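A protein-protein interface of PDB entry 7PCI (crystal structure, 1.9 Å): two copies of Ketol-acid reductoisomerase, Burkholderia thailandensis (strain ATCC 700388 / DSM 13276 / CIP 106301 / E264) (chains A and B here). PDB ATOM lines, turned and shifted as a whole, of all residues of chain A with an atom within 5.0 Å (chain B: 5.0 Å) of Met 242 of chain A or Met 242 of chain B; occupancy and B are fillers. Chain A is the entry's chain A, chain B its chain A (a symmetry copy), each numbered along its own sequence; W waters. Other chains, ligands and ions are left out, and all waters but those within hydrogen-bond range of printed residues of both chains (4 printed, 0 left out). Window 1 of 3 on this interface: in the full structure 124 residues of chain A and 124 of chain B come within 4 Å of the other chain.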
ATOM      1  N   LEU A 207     -21.095  23.506   3.519  1.00  0.00           N
ATOM      2  CA  LEU A 207     -21.578  22.789   4.728  1.00  0.00           C
ATOM      3  C   LEU A 207     -21.214  23.600   5.980  1.00  0.00           C
ATOM      4  O   LEU A 207     -22.113  23.835   6.810  1.00  0.00           O
ATOM      5  CB  LEU A 207     -20.958  21.390   4.737  1.00  0.00           C
ATOM      6  CG  LEU A 207     -21.618  20.380   5.669  1.00  0.00           C
ATOM      7  CD1 LEU A 207     -21.435  18.962   5.145  1.00  0.00           C
ATOM      8  CD2 LEU A 207     -21.063  20.508   7.077  1.00  0.00           C
ATOM      9  N   VAL A 211     -23.708  25.818   8.602  1.00  0.00           N
ATOM     10  CA  VAL A 211     -23.607  25.674  10.085  1.00  0.00           C
ATOM     11  C   VAL A 211     -23.357  27.059  10.689  1.00  0.00           C
ATOM     12  O   VAL A 211     -23.993  27.384  11.707  1.00  0.00           O
ATOM     13  CB  VAL A 211     -22.494  24.684  10.483  1.00  0.00           C
ATOM     14  CG1 VAL A 211     -22.189  24.730  11.970  1.00  0.00           C
ATOM     15  CG2 VAL A 211     -22.821  23.262  10.061  1.00  0.00           C
ATOM     16  N   VAL A 232     -25.892  23.684  16.171  1.00  0.00           N
ATOM     17  CA  VAL A 232     -25.499  23.743  14.732  1.00  0.00           C
ATOM     18  C   VAL A 232     -24.412  22.701  14.425  1.00  0.00           C
ATOM     19  O   VAL A 232     -24.358  22.266  13.264  1.00  0.00           O
ATOM     20  CB  VAL A 232     -25.105  25.166  14.289  1.00  0.00           C
ATOM     21  CG1 VAL A 232     -26.298  26.104  14.364  1.00  0.00           C
ATOM     22  CG2 VAL A 232     -23.923  25.724  15.067  1.00  0.00           C
ATOM     23  N   TYR A 233     -23.610  22.277  15.411  1.00  0.00           N
ATOM     24  CA  TYR A 233     -22.654  21.143  15.256  1.00  0.00           C
ATOM     25  C   TYR A 233     -21.991  20.739  16.582  1.00  0.00           C
ATOM     26  O   TYR A 233     -21.642  19.547  16.698  1.00  0.00           O
ATOM     27  CB  TYR A 233     -21.567  21.468  14.225  1.00  0.00           C
ATOM     28  CG  TYR A 233     -20.466  22.365  14.726  1.00  0.00           C
ATOM     29  CD1 TYR A 233     -20.620  23.741  14.745  1.00  0.00           C
ATOM     30  CD2 TYR A 233     -19.271  21.840  15.188  1.00  0.00           C
ATOM     31  CE1 TYR A 233     -19.617  24.575  15.210  1.00  0.00           C
ATOM     32  CE2 TYR A 233     -18.258  22.658  15.660  1.00  0.00           C
ATOM     33  CZ  TYR A 233     -18.432  24.030  15.671  1.00  0.00           C
ATOM     34  OH  TYR A 233     -17.439  24.842  16.133  1.00  0.00           O
ATOM     35  N   MET A 238     -25.506  16.865  14.715  1.00  0.00           N
ATOM     36  CA  MET A 238     -25.566  17.018  13.236  1.00  0.00           C
ATOM     37  C   MET A 238     -24.509  16.105  12.599  1.00  0.00           C
ATOM     38  O   MET A 238     -24.833  15.454  11.594  1.00  0.00           O
ATOM     39  CB  MET A 238     -25.356  18.474  12.812  1.00  0.00           C
ATOM     40  CG  MET A 238     -26.468  19.403  13.284  1.00  0.00           C
ATOM     41  SD  MET A 238     -28.147  18.807  12.922  1.00  0.00           S
ATOM     42  CE  MET A 238     -28.089  18.691  11.136  1.00  0.00           C
ATOM     43  N   GLY A 239     -23.315  16.023  13.196  1.00  0.00           N
ATOM     44  CA  GLY A 239     -22.253  15.084  12.781  1.00  0.00           C
ATOM     45  C   GLY A 239     -22.718  13.641  12.881  1.00  0.00           C
ATOM     46  O   GLY A 239     -22.438  12.860  11.947  1.00  0.00           O
ATOM     47  N   LYS A 240     -23.417  13.299  13.967  1.00  0.00           N
ATOM     48  CA  LYS A 240     -23.989  11.945  14.199  1.00  0.00           C
ATOM     49  C   LYS A 240     -25.051  11.655  13.130  1.00  0.00           C
ATOM     50  O   LYS A 240     -25.034  10.543  12.574  1.00  0.00           O
ATOM     51  CB  LYS A 240     -24.568  11.829  15.613  1.00  0.00           C
ATOM     52  CG  LYS A 240     -23.548  11.584  16.719  1.00  0.00           C
ATOM     53  CD  LYS A 240     -22.737  10.304  16.570  1.00  0.00           C
ATOM     54  CE  LYS A 240     -23.571   9.086  16.237  1.00  0.00           C
ATOM     55  NZ  LYS A 240     -22.797   7.833  16.411  1.00  0.00           N
ATOM     56  N   MET A 241     -25.929  12.622  12.847  1.00  0.00           N
ATOM     57  CA  MET A 241     -26.995  12.498  11.816  1.00  0.00           C
ATOM     58  C   MET A 241     -26.349  12.186  10.459  1.00  0.00           C
ATOM     59  O   MET A 241     -26.877  11.310   9.744  1.00  0.00           O
ATOM     60  CB  MET A 241     -27.827  13.780  11.707  1.00  0.00           C
ATOM     61  CG  MET A 241     -29.121  13.591  10.930  1.00  0.00           C
ATOM     62  SD  MET A 241     -29.872  15.130  10.331  1.00  0.00           S
ATOM     63  CE  MET A 241     -28.546  15.794   9.324  1.00  0.00           C
ATOM     64  N   MET A 242     -25.244  12.865  10.130  1.00  0.00           N
ATOM     65  CA  MET A 242     -24.522  12.715   8.836  1.00  0.00           C
ATOM     66  C   MET A 242     -23.814  11.354   8.772  1.00  0.00           C
ATOM     67  O   MET A 242     -23.822  10.740   7.687  1.00  0.00           O
ATOM     68  CB  MET A 242     -23.480  13.820   8.647  1.00  0.00           C
ATOM     69  CG  MET A 242     -24.076  15.181   8.374  1.00  0.00           C
ATOM     70  SD  MET A 242     -23.280  15.974   6.957  1.00  0.00           S
ATOM     71  CE  MET A 242     -24.064  15.083   5.616  1.00  0.00           C
ATOM     72  N   LEU A 243     -23.205  10.907   9.874  1.00  0.00           N
ATOM     73  CA  LEU A 243     -22.459   9.618   9.909  1.00  0.00           C
ATOM     74  C   LEU A 243     -23.451   8.447   9.940  1.00  0.00           C
ATOM     75  O   LEU A 243     -23.233   7.476   9.190  1.00  0.00           O
ATOM     76  CB  LEU A 243     -21.504   9.593  11.107  1.00  0.00           C
ATOM     77  CG  LEU A 243     -20.422   8.514  11.059  1.00  0.00           C
ATOM     78  CD1 LEU A 243     -19.570   8.628   9.799  1.00  0.00           C
ATOM     79  CD2 LEU A 243     -19.539   8.582  12.297  1.00  0.00           C
ATOM     80  N   ASP A 244     -24.501   8.533  10.761  1.00  0.00           N
ATOM     81  CA  ASP A 244     -25.618   7.547  10.770  1.00  0.00           C
ATOM     82  C   ASP A 244     -26.308   7.565   9.401  1.00  0.00           C
ATOM     83  O   ASP A 244     -26.709   6.480   8.931  1.00  0.00           O
ATOM     84  CB  ASP A 244     -26.617   7.831  11.896  1.00  0.00           C
ATOM     85  CG  ASP A 244     -26.089   7.496  13.278  1.00  0.00           C
ATOM     86  OD1 ASP A 244     -25.045   6.821  13.358  1.00  0.00           O
ATOM     87  OD2 ASP A 244     -26.729   7.912  14.263  1.00  0.00           O
ATOM     88  N   GLY A 245     -26.432   8.753   8.799  1.00  0.00           N
ATOM     89  CA  GLY A 245     -27.029   8.962   7.466  1.00  0.00           C
ATOM     90  C   GLY A 245     -26.225   8.273   6.379  1.00  0.00           C
ATOM     91  O   GLY A 245     -26.844   7.709   5.455  1.00  0.00           O
ATOM     92  N   ALA A 246     -24.891   8.319   6.480  1.00  0.00           N
ATOM     93  CA  ALA A 246     -23.953   7.629   5.564  1.00  0.00           C
ATOM     94  C   ALA A 246     -24.337   6.150   5.484  1.00  0.00           C
ATOM     95  O   ALA A 246     -24.259   5.581   4.381  1.00  0.00           O
ATOM     96  CB  ALA A 246     -22.526   7.808   6.020  1.00  0.00           C
ATOM     97  N   LEU A 250     -29.963   9.759   4.913  1.00  0.00           N
ATOM     98  CA  LEU A 250     -30.096  10.993   5.733  1.00  0.00           C
ATOM     99  C   LEU A 250     -31.561  11.207   6.127  1.00  0.00           C
ATOM    100  O   LEU A 250     -31.821  11.478   7.316  1.00  0.00           O
ATOM    101  CB  LEU A 250     -29.542  12.182   4.945  1.00  0.00           C
ATOM    102  CG  LEU A 250     -28.022  12.208   4.791  1.00  0.00           C
ATOM    103  CD1 LEU A 250     -27.605  13.140   3.664  1.00  0.00           C
ATOM    104  CD2 LEU A 250     -27.356  12.618   6.093  1.00  0.00           C
ATOM    105  N   LEU B 207     -28.917  21.278   5.312  1.00  0.00           N
ATOM    106  CA  LEU B 207     -27.709  20.413   5.300  1.00  0.00           C
ATOM    107  C   LEU B 207     -27.917  19.261   4.307  1.00  0.00           C
ATOM    108  O   LEU B 207     -27.027  19.047   3.461  1.00  0.00           O
ATOM    109  CB  LEU B 207     -27.460  19.916   6.727  1.00  0.00           C
ATOM    110  CG  LEU B 207     -26.074  19.342   6.995  1.00  0.00           C
ATOM    111  CD1 LEU B 207     -25.689  19.520   8.457  1.00  0.00           C
ATOM    112  CD2 LEU B 207     -26.016  17.877   6.600  1.00  0.00           C
ATOM    113  N   VAL B 211     -26.130  18.586   0.517  1.00  0.00           N
ATOM    114  CA  VAL B 211     -25.556  17.257   0.149  1.00  0.00           C
ATOM    115  C   VAL B 211     -26.224  16.784  -1.146  1.00  0.00           C
ATOM    116  O   VAL B 211     -25.508  16.286  -2.033  1.00  0.00           O
ATOM    117  CB  VAL B 211     -25.743  16.227   1.280  1.00  0.00           C
ATOM    118  CG1 VAL B 211     -25.421  14.812   0.829  1.00  0.00           C
ATOM    119  CG2 VAL B 211     -24.927  16.581   2.511  1.00  0.00           C
ATOM    120  N   VAL B 232     -20.418  13.022  -1.223  1.00  0.00           N
ATOM    121  CA  VAL B 232     -21.309  14.049  -0.607  1.00  0.00           C
ATOM    122  C   VAL B 232     -21.723  13.624   0.811  1.00  0.00           C
ATOM    123  O   VAL B 232     -21.993  14.530   1.615  1.00  0.00           O
ATOM    124  CB  VAL B 232     -22.514  14.396  -1.504  1.00  0.00           C
ATOM    125  CG1 VAL B 232     -22.055  15.058  -2.792  1.00  0.00           C
ATOM    126  CG2 VAL B 232     -23.401  13.195  -1.795  1.00  0.00           C
ATOM    127  N   TYR B 233     -21.735  12.324   1.130  1.00  0.00           N
ATOM    128  CA  TYR B 233     -21.943  11.826   2.521  1.00  0.00           C
ATOM    129  C   TYR B 233     -21.727  10.310   2.648  1.00  0.00           C
ATOM    130  O   TYR B 233     -21.335   9.887   3.755  1.00  0.00           O
ATOM    131  CB  TYR B 233     -23.343  12.182   3.036  1.00  0.00           C
ATOM    132  CG  TYR B 233     -24.450  11.300   2.524  1.00  0.00           C
ATOM    133  CD1 TYR B 233     -25.033  11.530   1.289  1.00  0.00           C
ATOM    134  CD2 TYR B 233     -24.914  10.230   3.270  1.00  0.00           C
ATOM    135  CE1 TYR B 233     -26.046  10.721   0.805  1.00  0.00           C
ATOM    136  CE2 TYR B 233     -25.925   9.408   2.801  1.00  0.00           C
ATOM    137  CZ  TYR B 233     -26.494   9.654   1.564  1.00  0.00           C
ATOM    138  OH  TYR B 233     -27.490   8.850   1.096  1.00  0.00           O
ATOM    139  N   MET B 238     -17.775  13.231   5.237  1.00  0.00           N
ATOM    140  CA  MET B 238     -18.383  14.537   5.611  1.00  0.00           C
ATOM    141  C   MET B 238     -18.970  14.424   7.025  1.00  0.00           C
ATOM    142  O   MET B 238     -18.779  15.364   7.811  1.00  0.00           O
ATOM    143  CB  MET B 238     -19.457  14.966   4.608  1.00  0.00           C
ATOM    144  CG  MET B 238     -18.901  15.249   3.218  1.00  0.00           C
ATOM    145  SD  MET B 238     -17.452  16.347   3.200  1.00  0.00           S
ATOM    146  CE  MET B 238     -18.131  17.820   3.959  1.00  0.00           C
ATOM    147  N   GLY B 239     -19.608  13.293   7.347  1.00  0.00           N
ATOM    148  CA  GLY B 239     -20.099  12.986   8.706  1.00  0.00           C
ATOM    149  C   GLY B 239     -18.963  12.965   9.715  1.00  0.00           C
ATOM    150  O   GLY B 239     -19.138  13.518  10.820  1.00  0.00           O
ATOM    151  N   LYS B 240     -17.830  12.360   9.345  1.00  0.00           N
ATOM    152  CA  LYS B 240     -16.606  12.292  10.189  1.00  0.00           C
ATOM    153  C   LYS B 240     -16.062  13.710  10.404  1.00  0.00           C
ATOM    154  O   LYS B 240     -15.720  14.039  11.553  1.00  0.00           O
ATOM    155  CB  LYS B 240     -15.554  11.375   9.558  1.00  0.00           C
ATOM    156  CG  LYS B 240     -15.777   9.882   9.768  1.00  0.00           C
ATOM    157  CD  LYS B 240     -15.798   9.436  11.224  1.00  0.00           C
ATOM    158  CE  LYS B 240     -14.664  10.000  12.053  1.00  0.00           C
ATOM    159  NZ  LYS B 240     -14.543   9.302  13.356  1.00  0.00           N
ATOM    160  N   MET B 241     -15.998  14.519   9.342  1.00  0.00           N
ATOM    161  CA  MET B 241     -15.520  15.928   9.401  1.00  0.00           C
ATOM    162  C   MET B 241     -16.382  16.710  10.401  1.00  0.00           C
ATOM    163  O   MET B 241     -15.806  17.482  11.195  1.00  0.00           O
ATOM    164  CB  MET B 241     -15.586  16.604   8.027  1.00  0.00           C
ATOM    165  CG  MET B 241     -14.801  17.906   7.962  1.00  0.00           C
ATOM    166  SD  MET B 241     -15.252  18.988   6.576  1.00  0.00           S
ATOM    167  CE  MET B 241     -16.998  19.242   6.888  1.00  0.00           C
ATOM    168  N   MET B 242     -17.703  16.504  10.373  1.00  0.00           N
ATOM    169  CA  MET B 242     -18.682  17.214  11.243  1.00  0.00           C
ATOM    170  C   MET B 242     -18.548  16.739  12.697  1.00  0.00           C
ATOM    171  O   MET B 242     -18.649  17.590  13.603  1.00  0.00           O
ATOM    172  CB  MET B 242     -20.120  16.973  10.778  1.00  0.00           C
ATOM    173  CG  MET B 242     -20.470  17.676   9.488  1.00  0.00           C
ATOM    174  SD  MET B 242     -22.038  18.567   9.629  1.00  0.00           S
ATOM    175  CE  MET B 242     -21.502  20.001  10.560  1.00  0.00           C
ATOM    176  N   LEU B 243     -18.356  15.436  12.920  1.00  0.00           N
ATOM    177  CA  LEU B 243     -18.250  14.866  14.292  1.00  0.00           C
ATOM    178  C   LEU B 243     -16.878  15.208  14.890  1.00  0.00           C
ATOM    179  O   LEU B 243     -16.837  15.614  16.066  1.00  0.00           O
ATOM    180  CB  LEU B 243     -18.500  13.355  14.258  1.00  0.00           C
ATOM    181  CG  LEU B 243     -18.792  12.709  15.612  1.00  0.00           C
ATOM    182  CD1 LEU B 243     -19.992  13.354  16.297  1.00  0.00           C
ATOM    183  CD2 LEU B 243     -19.020  11.212  15.456  1.00  0.00           C
ATOM    184  N   ASP B 244     -15.799  15.061  14.115  1.00  0.00           N
ATOM    185  CA  ASP B 244     -14.436  15.507  14.514  1.00  0.00           C
ATOM    186  C   ASP B 244     -14.450  17.026  14.719  1.00  0.00           C
ATOM    187  O   ASP B 244     -13.768  17.500  15.652  1.00  0.00           O
ATOM    188  CB  ASP B 244     -13.380  15.099  13.483  1.00  0.00           C
ATOM    189  CG  ASP B 244     -13.073  13.613  13.479  1.00  0.00           C
ATOM    190  OD1 ASP B 244     -13.493  12.927  14.430  1.00  0.00           O
ATOM    191  OD2 ASP B 244     -12.414  13.156  12.525  1.00  0.00           O
ATOM    192  N   GLY B 245     -15.200  17.746  13.877  1.00  0.00           N
ATOM    193  CA  GLY B 245     -15.370  19.210  13.944  1.00  0.00           C
ATOM    194  C   GLY B 245     -16.053  19.636  15.230  1.00  0.00           C
ATOM    195  O   GLY B 245     -15.649  20.670  15.797  1.00  0.00           O
ATOM    196  N   ALA B 246     -17.057  18.870  15.673  1.00  0.00           N
ATOM    197  CA  ALA B 246     -17.776  19.083  16.951  1.00  0.00           C
ATOM    198  C   ALA B 246     -16.754  19.167  18.086  1.00  0.00           C
ATOM    199  O   ALA B 246     -16.950  19.995  18.993  1.00  0.00           O
ATOM    200  CB  ALA B 246     -18.781  17.983  17.192  1.00  0.00           C
ATOM    201  N   LEU B 250     -14.529  22.983  13.036  1.00  0.00           N
ATOM    202  CA  LEU B 250     -14.744  22.504  11.643  1.00  0.00           C
ATOM    203  C   LEU B 250     -13.580  22.949  10.751  1.00  0.00           C
ATOM    204  O   LEU B 250     -13.058  22.106   9.995  1.00  0.00           O
ATOM    205  CB  LEU B 250     -16.085  23.033  11.131  1.00  0.00           C
ATOM    206  CG  LEU B 250     -17.320  22.386  11.755  1.00  0.00           C
ATOM    207  CD1 LEU B 250     -18.556  23.242  11.528  1.00  0.00           C
ATOM    208  CD2 LEU B 250     -17.533  20.987  11.202  1.00  0.00           C
HETATM  209  O   HOH W   1     -21.284  11.242   6.220  1.00  0.00           O
HETATM  210  O   HOH W   2     -21.418  17.592  14.688  1.00  0.00           O
HETATM  211  O   HOH W   3     -29.670   9.934   1.962  1.00  0.00           O
HETATM  212  O   HOH W   4     -15.993  25.359  14.055  1.00  0.00           O
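Along chain A the printed residues that touch a printed residue of chain B span positions 207 to 250. Of the 14 printed residues of chain B, 11 touch a printed residue of chain A. Among the printed residues, 24 pairs touch across the chains.
Water W4 lies within hydrogen-bond range of the side-chain hydroxyl of Tyr 233 of chain A (2.6 Å) and the backbone NH of Leu 250 of chain B (3.0 Å). Water W3 bridges OH of Tyr 233 of chain B (2.6 Å) and N of Leu 250 of chain A (3.0 Å). Water W2 lies within hydrogen-bond range of O of Tyr 233 of chain A, N of Gly 239 of chain A and O of Met 242 of chain B. Water W1 lies within hydrogen-bond range of O of Tyr 233 of chain B (2.8 Å), N of Gly 239 of chain B (2.9 Å) and O of Met 242 of chain A (3.0 Å).
The side-chain amino group (NZ) of Lys 240 of chain A lies within salt-bridge range of the side-chain carboxylate (OD1) of Asp 244 of chain A, at 3.9 Å. The side-chain amino group of Lys 240 of chain B is in salt-bridge range of the side-chain carboxylate of Asp 244 of chain B, at 3.9 Å.
Of the printed residues of chain B, Met 242 of chain A touches Leu 207 (3.4 Å), Val 211 (3.6 Å), Tyr 233 (3.9 Å), Gly 239 (3.5 Å) and Met 242 (3.9 Å). Met 242 of chain B touches just these residues of chain A: Leu 207, Val 211, Tyr 233, Gly 239 and Met 242. Of the printed residues of chain A, Lys 240 of chain B touches Leu 243. Of the printed residues of chain B, Leu 250 of chain A touches Val 211 (3.95 Å) and Tyr 233 (3.8 Å). Printed residues of chain B within 4 Å of Leu 243 of chain A: Gly 239 (3.9 Å) and Lys 240 (3.98 Å). Printed residues of chain B within 4 Å of Gly 239 of chain A: Gly 239 (3.5 Å), Met 242 (3.5 Å) and Leu 243 (3.9 Å). Asp 244 of chain B touches none of the printed residues of chain A. Asp 244 of chain A touches none of the printed residues of chain B. The nearest residue of chain B that does not touch Met 242 of chain A is Val 232 of chain B (4.5 Å). The nearest residue of chain A that does not touch Met 242 of chain B is Val 232 of chain A (4.5 Å). The nearest printed residue of chain B that does not touch Leu 207 of chain A is Met 241 of chain B (4.3 Å).
Leu 207 of chain A touches Met 238 of chain B, and with the chains exchanged Met 238 of chain A touches Leu 207 of chain B. Leu 207 of chain A touches Met 242 of chain B, and with the chains exchanged Met 242 of chain A touches Leu 207 of chain B. Val 211 of chain A touches Met 242 of chain B, and with the chains exchanged Met 242 of chain A touches Val 211 of chain B. Tyr 233 of chain A touches Gly 245 of chain B, and with the chains exchanged Gly 245 of chain A touches Tyr 233 of chain B. Of the 24 pairs that touch across the chains among the printed residues, 24 have their exchanged pair printed and touching as well.
Among the printed residues, pairs that only touch across the chains: Gly 245 of chain A with Tyr 233 of chain B (3.3 Å), Tyr 233 of chain A with Gly 245 of chain B (3.3 Å), Ala 246 of chain A with Tyr 233 of chain B (3.3 Å), Tyr 233 of chain A with Ala 246 of chain B (3.3 Å), Leu 207 of chain A with Met 242 of chain B (3.4 Å), Met 242 of chain A with Leu 207 of chain B (3.4 Å), Gly 239 of chain A with Met 242 of chain B (3.5 Å), Met 242 of chain A with Gly 239 of chain B (3.5 Å), Gly 239 of chain A with Gly 239 of chain B (3.5 Å), Val 211 of chain A with Met 242 of chain B (3.6 Å), Met 242 of chain A with Val 211 of chain B (3.6 Å), Met 238 of chain A with Leu 207 of chain B (3.7 Å), Leu 207 of chain A with Met 238 of chain B (3.7 Å), Leu 250 of chain A with Tyr 233 of chain B (3.8 Å), Tyr 233 of chain A with Leu 250 of chain B (3.8 Å), Gly 239 of chain A with Leu 243 of chain B (3.9 Å), Leu 243 of chain A with Gly 239 of chain B (3.9 Å), Met 242 of chain A with Met 242 of chain B (3.9 Å), Tyr 233 of chain A with Met 242 of chain B (3.9 Å), Met 242 of chain A with Tyr 233 of chain B (3.9 Å), Leu 250 of chain A with Val 211 of chain B (3.95 Å), Val 211 of chain A with Leu 250 of chain B (3.95 Å), Leu 243 of chain A with Lys 240 of chain B (3.98 Å) and Lys 240 of chain A with Leu 243 of chain B (3.99 Å).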
